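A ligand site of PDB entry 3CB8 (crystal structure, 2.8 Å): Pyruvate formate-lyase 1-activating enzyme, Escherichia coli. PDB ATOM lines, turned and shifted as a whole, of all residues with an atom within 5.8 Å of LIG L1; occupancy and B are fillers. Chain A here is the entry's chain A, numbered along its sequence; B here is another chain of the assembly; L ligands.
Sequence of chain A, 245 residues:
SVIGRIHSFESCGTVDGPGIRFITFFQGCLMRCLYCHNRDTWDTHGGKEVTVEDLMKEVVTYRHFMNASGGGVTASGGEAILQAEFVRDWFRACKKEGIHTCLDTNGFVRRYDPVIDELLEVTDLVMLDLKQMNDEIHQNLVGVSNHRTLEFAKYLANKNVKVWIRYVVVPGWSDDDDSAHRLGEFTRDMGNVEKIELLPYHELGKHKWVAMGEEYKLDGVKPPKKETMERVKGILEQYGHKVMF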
ATOM      1  N   CYS A  29      -8.095  32.230  23.120  1.00  0.00           N
ATOM      2  CA  CYS A  29      -9.090  31.882  22.122  1.00  0.00           C
ATOM      3  C   CYS A  29     -10.455  32.358  22.591  1.00  0.00           C
ATOM      4  O   CYS A  29     -10.813  32.224  23.756  1.00  0.00           O
ATOM      5  CB  CYS A  29      -9.115  30.380  21.884  1.00  0.00           C
ATOM      6  SG  CYS A  29     -10.187  29.943  20.496  1.00  0.00           S
ATOM      7  N   CYS A  33     -15.102  25.509  21.623  1.00  0.00           N
ATOM      8  CA  CYS A  33     -15.444  24.228  21.027  1.00  0.00           C
ATOM      9  C   CYS A  33     -15.474  23.191  22.137  1.00  0.00           C
ATOM     10  O   CYS A  33     -14.646  23.206  23.044  1.00  0.00           O
ATOM     11  CB  CYS A  33     -14.405  23.851  19.979  1.00  0.00           C
ATOM     12  SG  CYS A  33     -14.097  25.181  18.768  1.00  0.00           S
ATOM     13  N   TYR A  35     -14.861  20.049  21.841  1.00  0.00           N
ATOM     14  CA  TYR A  35     -13.838  19.033  21.631  1.00  0.00           C
ATOM     15  C   TYR A  35     -12.405  19.512  21.736  1.00  0.00           C
ATOM     16  O   TYR A  35     -11.455  18.715  21.669  1.00  0.00           O
ATOM     17  CB  TYR A  35     -14.062  18.364  20.278  1.00  0.00           C
ATOM     18  CG  TYR A  35     -14.105  19.331  19.123  1.00  0.00           C
ATOM     19  CD1 TYR A  35     -12.936  19.939  18.670  1.00  0.00           C
ATOM     20  CD2 TYR A  35     -15.313  19.664  18.515  1.00  0.00           C
ATOM     21  CE1 TYR A  35     -12.961  20.867  17.632  1.00  0.00           C
ATOM     22  CE2 TYR A  35     -15.346  20.587  17.466  1.00  0.00           C
ATOM     23  CZ  TYR A  35     -14.164  21.183  17.036  1.00  0.00           C
ATOM     24  OH  TYR A  35     -14.195  22.100  16.017  1.00  0.00           O
ATOM     25  N   CYS A  36     -12.248  20.824  21.903  1.00  0.00           N
ATOM     26  CA  CYS A  36     -10.940  21.451  22.022  1.00  0.00           C
ATOM     27  C   CYS A  36      -9.907  20.663  22.800  1.00  0.00           C
ATOM     28  O   CYS A  36     -10.073  20.420  24.004  1.00  0.00           O
ATOM     29  CB  CYS A  36     -11.069  22.815  22.686  1.00  0.00           C
ATOM     30  SG  CYS A  36      -9.500  23.696  22.619  1.00  0.00           S
ATOM     31  N   HIS A  37      -8.817  20.275  22.148  1.00  0.00           N
ATOM     32  CA  HIS A  37      -7.807  19.522  22.873  1.00  0.00           C
ATOM     33  C   HIS A  37      -6.756  20.424  23.517  1.00  0.00           C
ATOM     34  O   HIS A  37      -5.861  19.944  24.205  1.00  0.00           O
ATOM     35  CB  HIS A  37      -7.161  18.463  21.980  1.00  0.00           C
ATOM     36  CG  HIS A  37      -6.745  18.953  20.630  1.00  0.00           C
ATOM     37  ND1 HIS A  37      -6.602  18.110  19.545  1.00  0.00           N
ATOM     38  CD2 HIS A  37      -6.417  20.194  20.201  1.00  0.00           C
ATOM     39  CE1 HIS A  37      -6.203  18.811  18.498  1.00  0.00           C
ATOM     40  NE2 HIS A  37      -6.079  20.081  18.865  1.00  0.00           N
ATOM     41  N   ASN A  38      -6.875  21.732  23.308  1.00  0.00           N
ATOM     42  CA  ASN A  38      -5.949  22.673  23.934  1.00  0.00           C
ATOM     43  C   ASN A  38      -6.769  23.589  24.810  1.00  0.00           C
ATOM     44  O   ASN A  38      -6.725  24.811  24.645  1.00  0.00           O
ATOM     45  CB  ASN A  38      -5.224  23.558  22.907  1.00  0.00           C
ATOM     46  CG  ASN A  38      -4.545  22.763  21.830  1.00  0.00           C
ATOM     47  OD1 ASN A  38      -3.827  21.796  22.103  1.00  0.00           O
ATOM     48  ND2 ASN A  38      -4.759  23.173  20.583  1.00  0.00           N
ATOM     49  N   SER A  76      -0.743  28.744  15.072  1.00  0.00           N
ATOM     50  CA  SER A  76      -1.917  28.046  15.576  1.00  0.00           C
ATOM     51  C   SER A  76      -2.068  28.273  17.076  1.00  0.00           C
ATOM     52  O   SER A  76      -1.942  29.397  17.559  1.00  0.00           O
ATOM     53  CB  SER A  76      -1.746  26.558  15.265  1.00  0.00           C
ATOM     54  OG  SER A  76      -2.915  25.823  15.587  1.00  0.00           O
ATOM     55  N   GLY A  77      -2.351  27.191  17.816  1.00  0.00           N
ATOM     56  CA  GLY A  77      -2.495  27.259  19.269  1.00  0.00           C
ATOM     57  C   GLY A  77      -3.938  27.382  19.697  1.00  0.00           C
ATOM     58  O   GLY A  77      -4.671  26.400  19.766  1.00  0.00           O
ATOM     59  N   GLY A  78      -4.293  28.616  20.043  1.00  0.00           N
ATOM     60  CA  GLY A  78      -5.641  28.973  20.401  1.00  0.00           C
ATOM     61  C   GLY A  78      -6.004  29.690  19.114  1.00  0.00           C
ATOM     62  O   GLY A  78      -6.012  29.054  18.060  1.00  0.00           O
ATOM     63  N   GLU A  79      -6.271  30.991  19.176  1.00  0.00           N
ATOM     64  CA  GLU A  79      -6.576  31.730  17.967  1.00  0.00           C
ATOM     65  C   GLU A  79      -5.507  32.759  17.645  1.00  0.00           C
ATOM     66  O   GLU A  79      -5.503  33.869  18.198  1.00  0.00           O
ATOM     67  CB  GLU A  79      -7.941  32.412  18.040  1.00  0.00           C
ATOM     68  CG  GLU A  79      -8.294  33.077  16.717  1.00  0.00           C
ATOM     69  CD  GLU A  79      -7.973  32.181  15.507  1.00  0.00           C
ATOM     70  OE1 GLU A  79      -7.673  32.720  14.416  1.00  0.00           O
ATOM     71  OE2 GLU A  79      -8.024  30.937  15.638  1.00  0.00           O
ATOM     72  N   ASP A 104      -3.186  28.685  10.798  1.00  0.00           N
ATOM     73  CA  ASP A 104      -4.247  27.756  11.197  1.00  0.00           C
ATOM     74  C   ASP A 104      -5.268  28.461  12.075  1.00  0.00           C
ATOM     75  O   ASP A 104      -5.086  28.584  13.282  1.00  0.00           O
ATOM     76  CB  ASP A 104      -3.636  26.583  11.964  1.00  0.00           C
ATOM     77  CG  ASP A 104      -4.617  25.472  12.206  1.00  0.00           C
ATOM     78  OD1 ASP A 104      -5.780  25.602  11.760  1.00  0.00           O
ATOM     79  OD2 ASP A 104      -4.227  24.460  12.830  1.00  0.00           O
ATOM     80  N   THR A 105      -6.379  28.897  11.478  1.00  0.00           N
ATOM     81  CA  THR A 105      -7.375  29.672  12.211  1.00  0.00           C
ATOM     82  C   THR A 105      -8.852  29.220  12.180  1.00  0.00           C
ATOM     83  O   THR A 105      -9.241  28.336  11.430  1.00  0.00           O
ATOM     84  CB  THR A 105      -7.279  31.158  11.740  1.00  0.00           C
ATOM     85  OG1 THR A 105      -8.330  31.946  12.319  1.00  0.00           O
ATOM     86  CG2 THR A 105      -7.391  31.236  10.236  1.00  0.00           C
ATOM     87  N   ASN A 106      -9.651  29.854  13.037  1.00  0.00           N
ATOM     88  CA  ASN A 106     -11.081  29.601  13.117  1.00  0.00           C
ATOM     89  C   ASN A 106     -11.822  30.744  12.394  1.00  0.00           C
ATOM     90  O   ASN A 106     -13.051  30.759  12.282  1.00  0.00           O
ATOM     91  CB  ASN A 106     -11.532  29.527  14.586  1.00  0.00           C
ATOM     92  CG  ASN A 106     -11.185  30.779  15.363  1.00  0.00           C
ATOM     93  OD1 ASN A 106     -11.296  31.897  14.859  1.00  0.00           O
ATOM     94  ND2 ASN A 106     -10.790  30.602  16.614  1.00  0.00           N
ATOM     95  N   MET A 127      -5.381  27.425   6.784  1.00  0.00           N
ATOM     96  CA  MET A 127      -6.208  26.270   7.052  1.00  0.00           C
ATOM     97  C   MET A 127      -7.344  26.831   7.883  1.00  0.00           C
ATOM     98  O   MET A 127      -7.241  26.998   9.099  1.00  0.00           O
ATOM     99  CB  MET A 127      -5.420  25.229   7.820  1.00  0.00           C
ATOM    100  CG  MET A 127      -4.282  24.702   7.002  1.00  0.00           C
ATOM    101  SD  MET A 127      -3.519  23.319   7.825  1.00  0.00           S
ATOM    102  CE  MET A 127      -2.549  24.182   9.094  1.00  0.00           C
ATOM    103  N   ASP A 129     -10.931  26.687   9.512  1.00  0.00           N
ATOM    104  CA  ASP A 129     -11.823  25.712  10.088  1.00  0.00           C
ATOM    105  C   ASP A 129     -13.250  26.159   9.914  1.00  0.00           C
ATOM    106  O   ASP A 129     -13.573  27.315  10.160  1.00  0.00           O
ATOM    107  CB  ASP A 129     -11.573  25.564  11.572  1.00  0.00           C
ATOM    108  CG  ASP A 129     -10.902  24.276  11.921  1.00  0.00           C
ATOM    109  OD1 ASP A 129      -9.716  24.102  11.536  1.00  0.00           O
ATOM    110  OD2 ASP A 129     -11.555  23.438  12.590  1.00  0.00           O
ATOM    111  N   LYS A 131     -16.468  24.797  11.410  1.00  0.00           N
ATOM    112  CA  LYS A 131     -16.913  23.825  12.385  1.00  0.00           C
ATOM    113  C   LYS A 131     -18.353  23.331  12.253  1.00  0.00           C
ATOM    114  O   LYS A 131     -18.661  22.224  12.687  1.00  0.00           O
ATOM    115  CB  LYS A 131     -16.636  24.391  13.794  1.00  0.00           C
ATOM    116  CG  LYS A 131     -15.138  24.587  14.010  1.00  0.00           C
ATOM    117  CD  LYS A 131     -14.776  25.411  15.231  1.00  0.00           C
ATOM    118  CE  LYS A 131     -13.259  25.654  15.305  1.00  0.00           C
ATOM    119  NZ  LYS A 131     -12.446  24.431  15.539  1.00  0.00           N
ATOM    120  N   ARG A 166     -10.883  22.922   6.961  1.00  0.00           N
ATOM    121  CA  ARG A 166     -10.755  21.803   7.876  1.00  0.00           C
ATOM    122  C   ARG A 166     -12.106  21.603   8.534  1.00  0.00           C
ATOM    123  O   ARG A 166     -12.707  22.545   9.071  1.00  0.00           O
ATOM    124  CB  ARG A 166      -9.684  22.066   8.932  1.00  0.00           C
ATOM    125  CG  ARG A 166      -8.352  21.438   8.592  1.00  0.00           C
ATOM    126  CD  ARG A 166      -7.280  21.793   9.619  1.00  0.00           C
ATOM    127  NE  ARG A 166      -6.032  21.073   9.398  1.00  0.00           N
ATOM    128  CZ  ARG A 166      -4.975  21.132  10.202  1.00  0.00           C
ATOM    129  NH1 ARG A 166      -3.877  20.438   9.931  1.00  0.00           N
ATOM    130  NH2 ARG A 166      -5.014  21.899  11.279  1.00  0.00           N
ATOM    131  N   VAL A 168     -13.716  19.205  11.338  1.00  0.00           N
ATOM    132  CA  VAL A 168     -13.576  18.169  12.345  1.00  0.00           C
ATOM    133  C   VAL A 168     -14.899  17.435  12.485  1.00  0.00           C
ATOM    134  O   VAL A 168     -15.908  18.017  12.835  1.00  0.00           O
ATOM    135  CB  VAL A 168     -13.172  18.757  13.716  1.00  0.00           C
ATOM    136  CG1 VAL A 168     -13.377  17.719  14.817  1.00  0.00           C
ATOM    137  CG2 VAL A 168     -11.723  19.176  13.668  1.00  0.00           C
ATOM    138  N   LEU A 199     -11.124  15.932   9.747  1.00  0.00           N
ATOM    139  CA  LEU A 199     -10.424  15.513  10.949  1.00  0.00           C
ATOM    140  C   LEU A 199     -11.340  14.790  11.886  1.00  0.00           C
ATOM    141  O   LEU A 199     -12.330  15.346  12.355  1.00  0.00           O
ATOM    142  CB  LEU A 199      -9.834  16.724  11.687  1.00  0.00           C
ATOM    143  CG  LEU A 199      -8.974  17.676  10.876  1.00  0.00           C
ATOM    144  CD1 LEU A 199      -8.603  18.860  11.730  1.00  0.00           C
ATOM    145  CD2 LEU A 199      -7.739  16.962  10.364  1.00  0.00           C
ATOM    146  N   PRO A 200     -11.021  13.527  12.199  1.00  0.00           N
ATOM    147  CA  PRO A 200     -11.813  12.694  13.106  1.00  0.00           C
ATOM    148  C   PRO A 200     -11.643  13.190  14.527  1.00  0.00           C
ATOM    149  O   PRO A 200     -10.539  13.519  14.958  1.00  0.00           O
ATOM    150  CB  PRO A 200     -11.207  11.314  12.920  1.00  0.00           C
ATOM    151  CG  PRO A 200      -9.775  11.618  12.693  1.00  0.00           C
ATOM    152  CD  PRO A 200      -9.850  12.773  11.708  1.00  0.00           C
ATOM    153  N   TYR A 201     -12.748  13.274  15.259  1.00  0.00           N
ATOM    154  CA  TYR A 201     -12.655  13.718  16.621  1.00  0.00           C
ATOM    155  C   TYR A 201     -11.871  12.694  17.413  1.00  0.00           C
ATOM    156  O   TYR A 201     -11.942  11.489  17.130  1.00  0.00           O
ATOM    157  CB  TYR A 201     -14.042  13.866  17.223  1.00  0.00           C
ATOM    158  CG  TYR A 201     -14.039  13.737  18.712  1.00  0.00           C
ATOM    159  CD1 TYR A 201     -14.263  12.493  19.315  1.00  0.00           C
ATOM    160  CD2 TYR A 201     -13.807  14.836  19.523  1.00  0.00           C
ATOM    161  CE1 TYR A 201     -14.255  12.363  20.695  1.00  0.00           C
ATOM    162  CE2 TYR A 201     -13.800  14.712  20.910  1.00  0.00           C
ATOM    163  CZ  TYR A 201     -14.037  13.482  21.490  1.00  0.00           C
ATOM    164  OH  TYR A 201     -14.055  13.365  22.857  1.00  0.00           O
ATOM    165  N   HIS A 202     -11.125  13.165  18.403  1.00  0.00           N
ATOM    166  CA  HIS A 202     -10.320  12.287  19.253  1.00  0.00           C
ATOM    167  C   HIS A 202     -10.406  12.759  20.685  1.00  0.00           C
ATOM    168  O   HIS A 202     -10.411  13.971  20.942  1.00  0.00           O
ATOM    169  CB  HIS A 202      -8.872  12.298  18.805  1.00  0.00           C
ATOM    170  CG  HIS A 202      -8.302  13.679  18.677  1.00  0.00           C
ATOM    171  ND1 HIS A 202      -8.047  14.276  17.465  1.00  0.00           N
ATOM    172  CD2 HIS A 202      -7.956  14.587  19.627  1.00  0.00           C
ATOM    173  CE1 HIS A 202      -7.568  15.490  17.656  1.00  0.00           C
ATOM    174  NE2 HIS A 202      -7.509  15.702  18.957  1.00  0.00           N
ATOM    175  N   GLU A 203     -10.503  11.842  21.627  1.00  0.00           N
ATOM    176  CA  GLU A 203     -10.547  12.245  23.013  1.00  0.00           C
ATOM    177  C   GLU A 203      -9.092  12.487  23.352  1.00  0.00           C
ATOM    178  O   GLU A 203      -8.258  11.586  23.222  1.00  0.00           O
ATOM    179  CB  GLU A 203     -11.137  11.147  23.900  1.00  0.00           C
ATOM    180  CG  GLU A 203     -11.240  11.524  25.385  1.00  0.00           C
ATOM    181  CD  GLU A 203     -12.318  10.728  26.120  1.00  0.00           C
ATOM    182  OE1 GLU A 203     -12.354  10.787  27.371  1.00  0.00           O
ATOM    183  OE2 GLU A 203     -13.139  10.058  25.448  1.00  0.00           O
ATOM    184  N   LEU A 204      -8.778  13.714  23.724  1.00  0.00           N
ATOM    185  CA  LEU A 204      -7.416  14.077  24.051  1.00  0.00           C
ATOM    186  C   LEU A 204      -7.401  15.544  24.398  1.00  0.00           C
ATOM    187  O   LEU A 204      -7.963  16.364  23.668  1.00  0.00           O
ATOM    188  CB  LEU A 204      -6.497  13.842  22.861  1.00  0.00           C
ATOM    189  CG  LEU A 204      -5.283  12.965  23.167  1.00  0.00           C
ATOM    190  CD1 LEU A 204      -4.376  12.953  21.952  1.00  0.00           C
ATOM    191  CD2 LEU A 204      -4.532  13.492  24.390  1.00  0.00           C
ATOM    192  N   TYR A 216     -15.559  17.891  30.865  1.00  0.00           N
ATOM    193  CA  TYR A 216     -15.408  17.596  29.451  1.00  0.00           C
ATOM    194  C   TYR A 216     -16.689  16.880  29.028  1.00  0.00           C
ATOM    195  O   TYR A 216     -16.867  15.696  29.298  1.00  0.00           O
ATOM    196  CB  TYR A 216     -14.188  16.698  29.230  1.00  0.00           C
ATOM    197  CG  TYR A 216     -13.892  16.409  27.780  1.00  0.00           C
ATOM    198  CD1 TYR A 216     -14.024  15.126  27.261  1.00  0.00           C
ATOM    199  CD2 TYR A 216     -13.456  17.419  26.912  1.00  0.00           C
ATOM    200  CE1 TYR A 216     -13.753  14.846  25.924  1.00  0.00           C
ATOM    201  CE2 TYR A 216     -13.181  17.161  25.573  1.00  0.00           C
ATOM    202  CZ  TYR A 216     -13.330  15.875  25.079  1.00  0.00           C
ATOM    203  OH  TYR A 216     -13.072  15.615  23.764  1.00  0.00           O
ATOM    204  N   SER B   2      -3.442  16.326  14.906  1.00  0.00           N
ATOM    205  CA  SER B   2      -3.502  17.643  14.277  1.00  0.00           C
ATOM    206  C   SER B   2      -3.891  18.791  15.200  1.00  0.00           C
ATOM    207  O   SER B   2      -5.011  18.840  15.707  1.00  0.00           O
ATOM    208  CB  SER B   2      -4.462  17.612  13.081  1.00  0.00           C
ATOM    209  OG  SER B   2      -3.915  16.891  11.996  1.00  0.00           O
ATOM    210  N   GLY B   3      -2.953  19.704  15.402  1.00  0.00           N
ATOM    211  CA  GLY B   3      -3.206  20.861  16.236  1.00  0.00           C
ATOM    212  C   GLY B   3      -3.130  20.594  17.722  1.00  0.00           C
ATOM    213  O   GLY B   3      -3.625  21.396  18.508  1.00  0.00           O
ATOM    214  N   TYR B   4      -2.506  19.483  18.124  1.00  0.00           N
ATOM    215  CA  TYR B   4      -2.410  19.196  19.553  1.00  0.00           C
ATOM    216  C   TYR B   4      -1.147  19.767  20.177  1.00  0.00           C
ATOM    217  O   TYR B   4      -0.037  19.321  19.890  1.00  0.00           O
ATOM    218  CB  TYR B   4      -2.459  17.688  19.811  1.00  0.00           C
ATOM    219  CG  TYR B   4      -2.436  17.328  21.282  1.00  0.00           C
ATOM    220  CD1 TYR B   4      -1.318  16.715  21.859  1.00  0.00           C
ATOM    221  CD2 TYR B   4      -3.522  17.609  22.110  1.00  0.00           C
ATOM    222  CE1 TYR B   4      -1.283  16.384  23.212  1.00  0.00           C
ATOM    223  CE2 TYR B   4      -3.501  17.278  23.475  1.00  0.00           C
ATOM    224  CZ  TYR B   4      -2.384  16.664  24.014  1.00  0.00           C
ATOM    225  OH  TYR B   4      -2.360  16.315  25.354  1.00  0.00           O
HETATM  226  N1  LIG L   1      -8.400  27.681  17.218  1.00  0.00           N
HETATM  227  C1  LIG L   1      -8.040  27.359  15.824  1.00  0.00           C
HETATM  228  C2  LIG L   1      -9.012  26.293  15.269  1.00  0.00           C
HETATM  229  O1  LIG L   1      -9.630  25.587  16.095  1.00  0.00           O
HETATM  230  O2  LIG L   1      -9.124  26.235  14.024  1.00  0.00           O
HETATM  231  C3  LIG L   1      -6.577  26.878  15.779  1.00  0.00           C
HETATM  232  C4  LIG L   1      -6.255  25.965  16.979  1.00  0.00           C
HETATM  233  S1  LIG L   1      -7.071  24.344  16.841  1.00  0.00           S
HETATM  234  C5  LIG L   1      -7.034  23.511  18.467  1.00  0.00           C
HETATM  235  C6  LIG L   1      -6.176  23.340  15.593  1.00  0.00           C
HETATM  236  C7  LIG L   1      -7.021  22.200  14.971  1.00  0.00           C
HETATM  237  O3  LIG L   1      -7.336  21.191  15.988  1.00  0.00           O
HETATM  238  C8  LIG L   1      -8.376  22.714  14.449  1.00  0.00           C
HETATM  239  O4  LIG L   1      -8.599  22.134  13.156  1.00  0.00           O
HETATM  240  C9  LIG L   1      -9.352  22.172  15.496  1.00  0.00           C
HETATM  241  O5  LIG L   1     -10.643  22.030  14.921  1.00  0.00           O
HETATM  242  C10 LIG L   1      -8.713  20.805  15.750  1.00  0.00           C
HETATM  243  N2  LIG L   1      -9.247  20.106  16.976  1.00  0.00           N
HETATM  244  C11 LIG L   1      -9.379  20.644  18.206  1.00  0.00           C
HETATM  245  N3  LIG L   1      -9.830  19.718  19.061  1.00  0.00           N
HETATM  246  C12 LIG L   1      -9.985  18.584  18.383  1.00  0.00           C
HETATM  247  C13 LIG L   1     -10.413  17.305  18.727  1.00  0.00           C
HETATM  248  N4  LIG L   1     -10.765  17.021  19.987  1.00  0.00           N
HETATM  249  N5  LIG L   1     -10.458  16.327  17.778  1.00  0.00           N
HETATM  250  C14 LIG L   1     -10.097  16.589  16.510  1.00  0.00           C
HETATM  251  N6  LIG L   1      -9.685  17.815  16.152  1.00  0.00           N
HETATM  252  C15 LIG L   1      -9.615  18.820  17.061  1.00  0.00           C
HETATM  253 FE1  LG2 L   2     -11.975  25.803  19.224  1.00  0.00          FE
HETATM  254 FE2  LG2 L   2      -9.462  26.046  18.160  1.00  0.00          FE
HETATM  255 FE3  LG2 L   2      -9.930  25.121  20.853  1.00  0.00          FE
HETATM  256 FE4  LG2 L   2     -10.362  27.746  20.120  1.00  0.00          FE
HETATM  257  S1  LG2 L   2      -8.356  26.617  20.111  1.00  0.00           S
HETATM  258  S2  LG2 L   2     -11.722  26.414  21.426  1.00  0.00           S
HETATM  259  S3  LG2 L   2     -11.189  27.568  17.995  1.00  0.00           S
HETATM  260  S4  LG2 L   2     -10.479  24.094  18.876  1.00  0.00           S
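FE3 of LG2 L2 is bound by SG of Cys 36, at 2.3 Å.
The side-chain sulfur (SG) of Cys 33 binds an iron atom (FE1) of LG2 L2, 2.3 Å away.
An oxygen (O4) of LIG L1 sits at hydrogen-bond distance from the side-chain carboxylate (OD1) of Asp 129, 2.8 Å away.
A nitrogen (N5) of LIG L1 lies close to a ring nitrogen (ND1) of His 202 (3.2 Å).
A nitrogen (N3) of LIG L1 is in hydrogen-bond range of the backbone NH of His 37, 3.3 Å away.
N of His 202 lies close to N5 of LIG L1, at 3.3 Å.
FE4 of LG2 L2 is bound by SG of Cys 29 (2.2 Å).
The side-chain amide nitrogen (ND2) of Asn 106 sits close to a sulfur (S3) of LG2 L2.
An oxygen (O3) of LIG L1 sits at hydrogen-bond distance from a ring nitrogen (NE2) of His 37 (3.3 Å).
N4 of LIG L1 lies within hydrogen-bond range of O of His 202, at 3.2 Å.
A nitrogen (N4) of LIG L1 is in hydrogen-bond range of the backbone carbonyl oxygen (O) of Tyr 35, 2.5 Å away.
The backbone NH of Cys 33 sits close to a sulfur (S2) of LG2 L2 (3.5 Å).
The backbone carbonyl oxygen (O) of Gly 78 lies close to a nitrogen (N1) of LIG L1, at 2.9 Å.
The side-chain carboxylate (OE2) of Glu 79 lies close to a nitrogen (N1) of LIG L1.
NZ of Lys 131 sits at hydrogen-bond distance from O5 of LIG L1 (3.1 Å).
O2 of LIG L1 sits close to O of Thr 105 (3.3 Å).
The backbone carbonyl oxygen (O) of Ser 2 of chain B sits close to an oxygen (O3) of LIG L1 (3.3 Å).
Merely in contact with LIG L1: Cys 36 (3.6 Å), Asn 38 (3.1 Å), Ser 76 (3.6 Å), Gly 77 (3.2 Å), Asp 104 (3.4 Å), Asn 106 (3.8 Å), Arg 166 (3.8 Å), Val 168 (3.3 Å), Leu 199 (3.6 Å), Pro 200 (3.5 Å), Tyr 201 (3.6 Å) and Gly 3 of chain B (3.9 Å).
Hydrophobic or aromatic side chains that line LIG L1: Tyr 35, His 37, Val 168, Leu 199, Tyr 201 and His 202.
Within 4 Å of LIG L1: Tyr 35, Cys 36, His 37, Asn 38, Ser 76, Gly 77, Gly 78, Glu 79, Asp 104, Thr 105, Asn 106, Asp 129, Lys 131, Arg 166, Val 168, Leu 199, Pro 200, Tyr 201, His 202, Ser 2 of chain B and Gly 3 of chain B.
The nearest printed residue that does not touch LIG L1 is Cys 29 (4.4 Å).
The side-chain amide nitrogen (ND2) of Asn 38 lies within hydrogen-bond range of the backbone carbonyl oxygen (O) of Gly 3 of chain B (3.0 Å).
The side-chain sulfur (SD) of Met 127 sits close to the guanidinium group (NH1) of Arg 166 (3.6 Å).
The side-chain amino group of Lys 131 lies within hydrogen-bond range of the side-chain hydroxyl of Tyr 35 (3.0 Å).
The backbone NH of Thr 105 lies within hydrogen-bond range of the backbone carbonyl oxygen of Met 127 (3.2 Å).
The backbone NH (N) of Asp 129 is in hydrogen-bond range of the backbone carbonyl oxygen (O) of Thr 105, 3.0 Å away.
OE2 of Glu 79 lies close to OG1 of Thr 105.
ND2 of Asn 106 is in hydrogen-bond range of OE2 of Glu 79.
The backbone carbonyl oxygen (O) of Gly 77 sits at hydrogen-bond distance from the side-chain amide nitrogen (ND2) of Asn 38, at 3.3 Å.
An oxygen (O1) of LIG L1 is bound to an iron atom (FE2) of LG2 L2 (2.1 Å).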
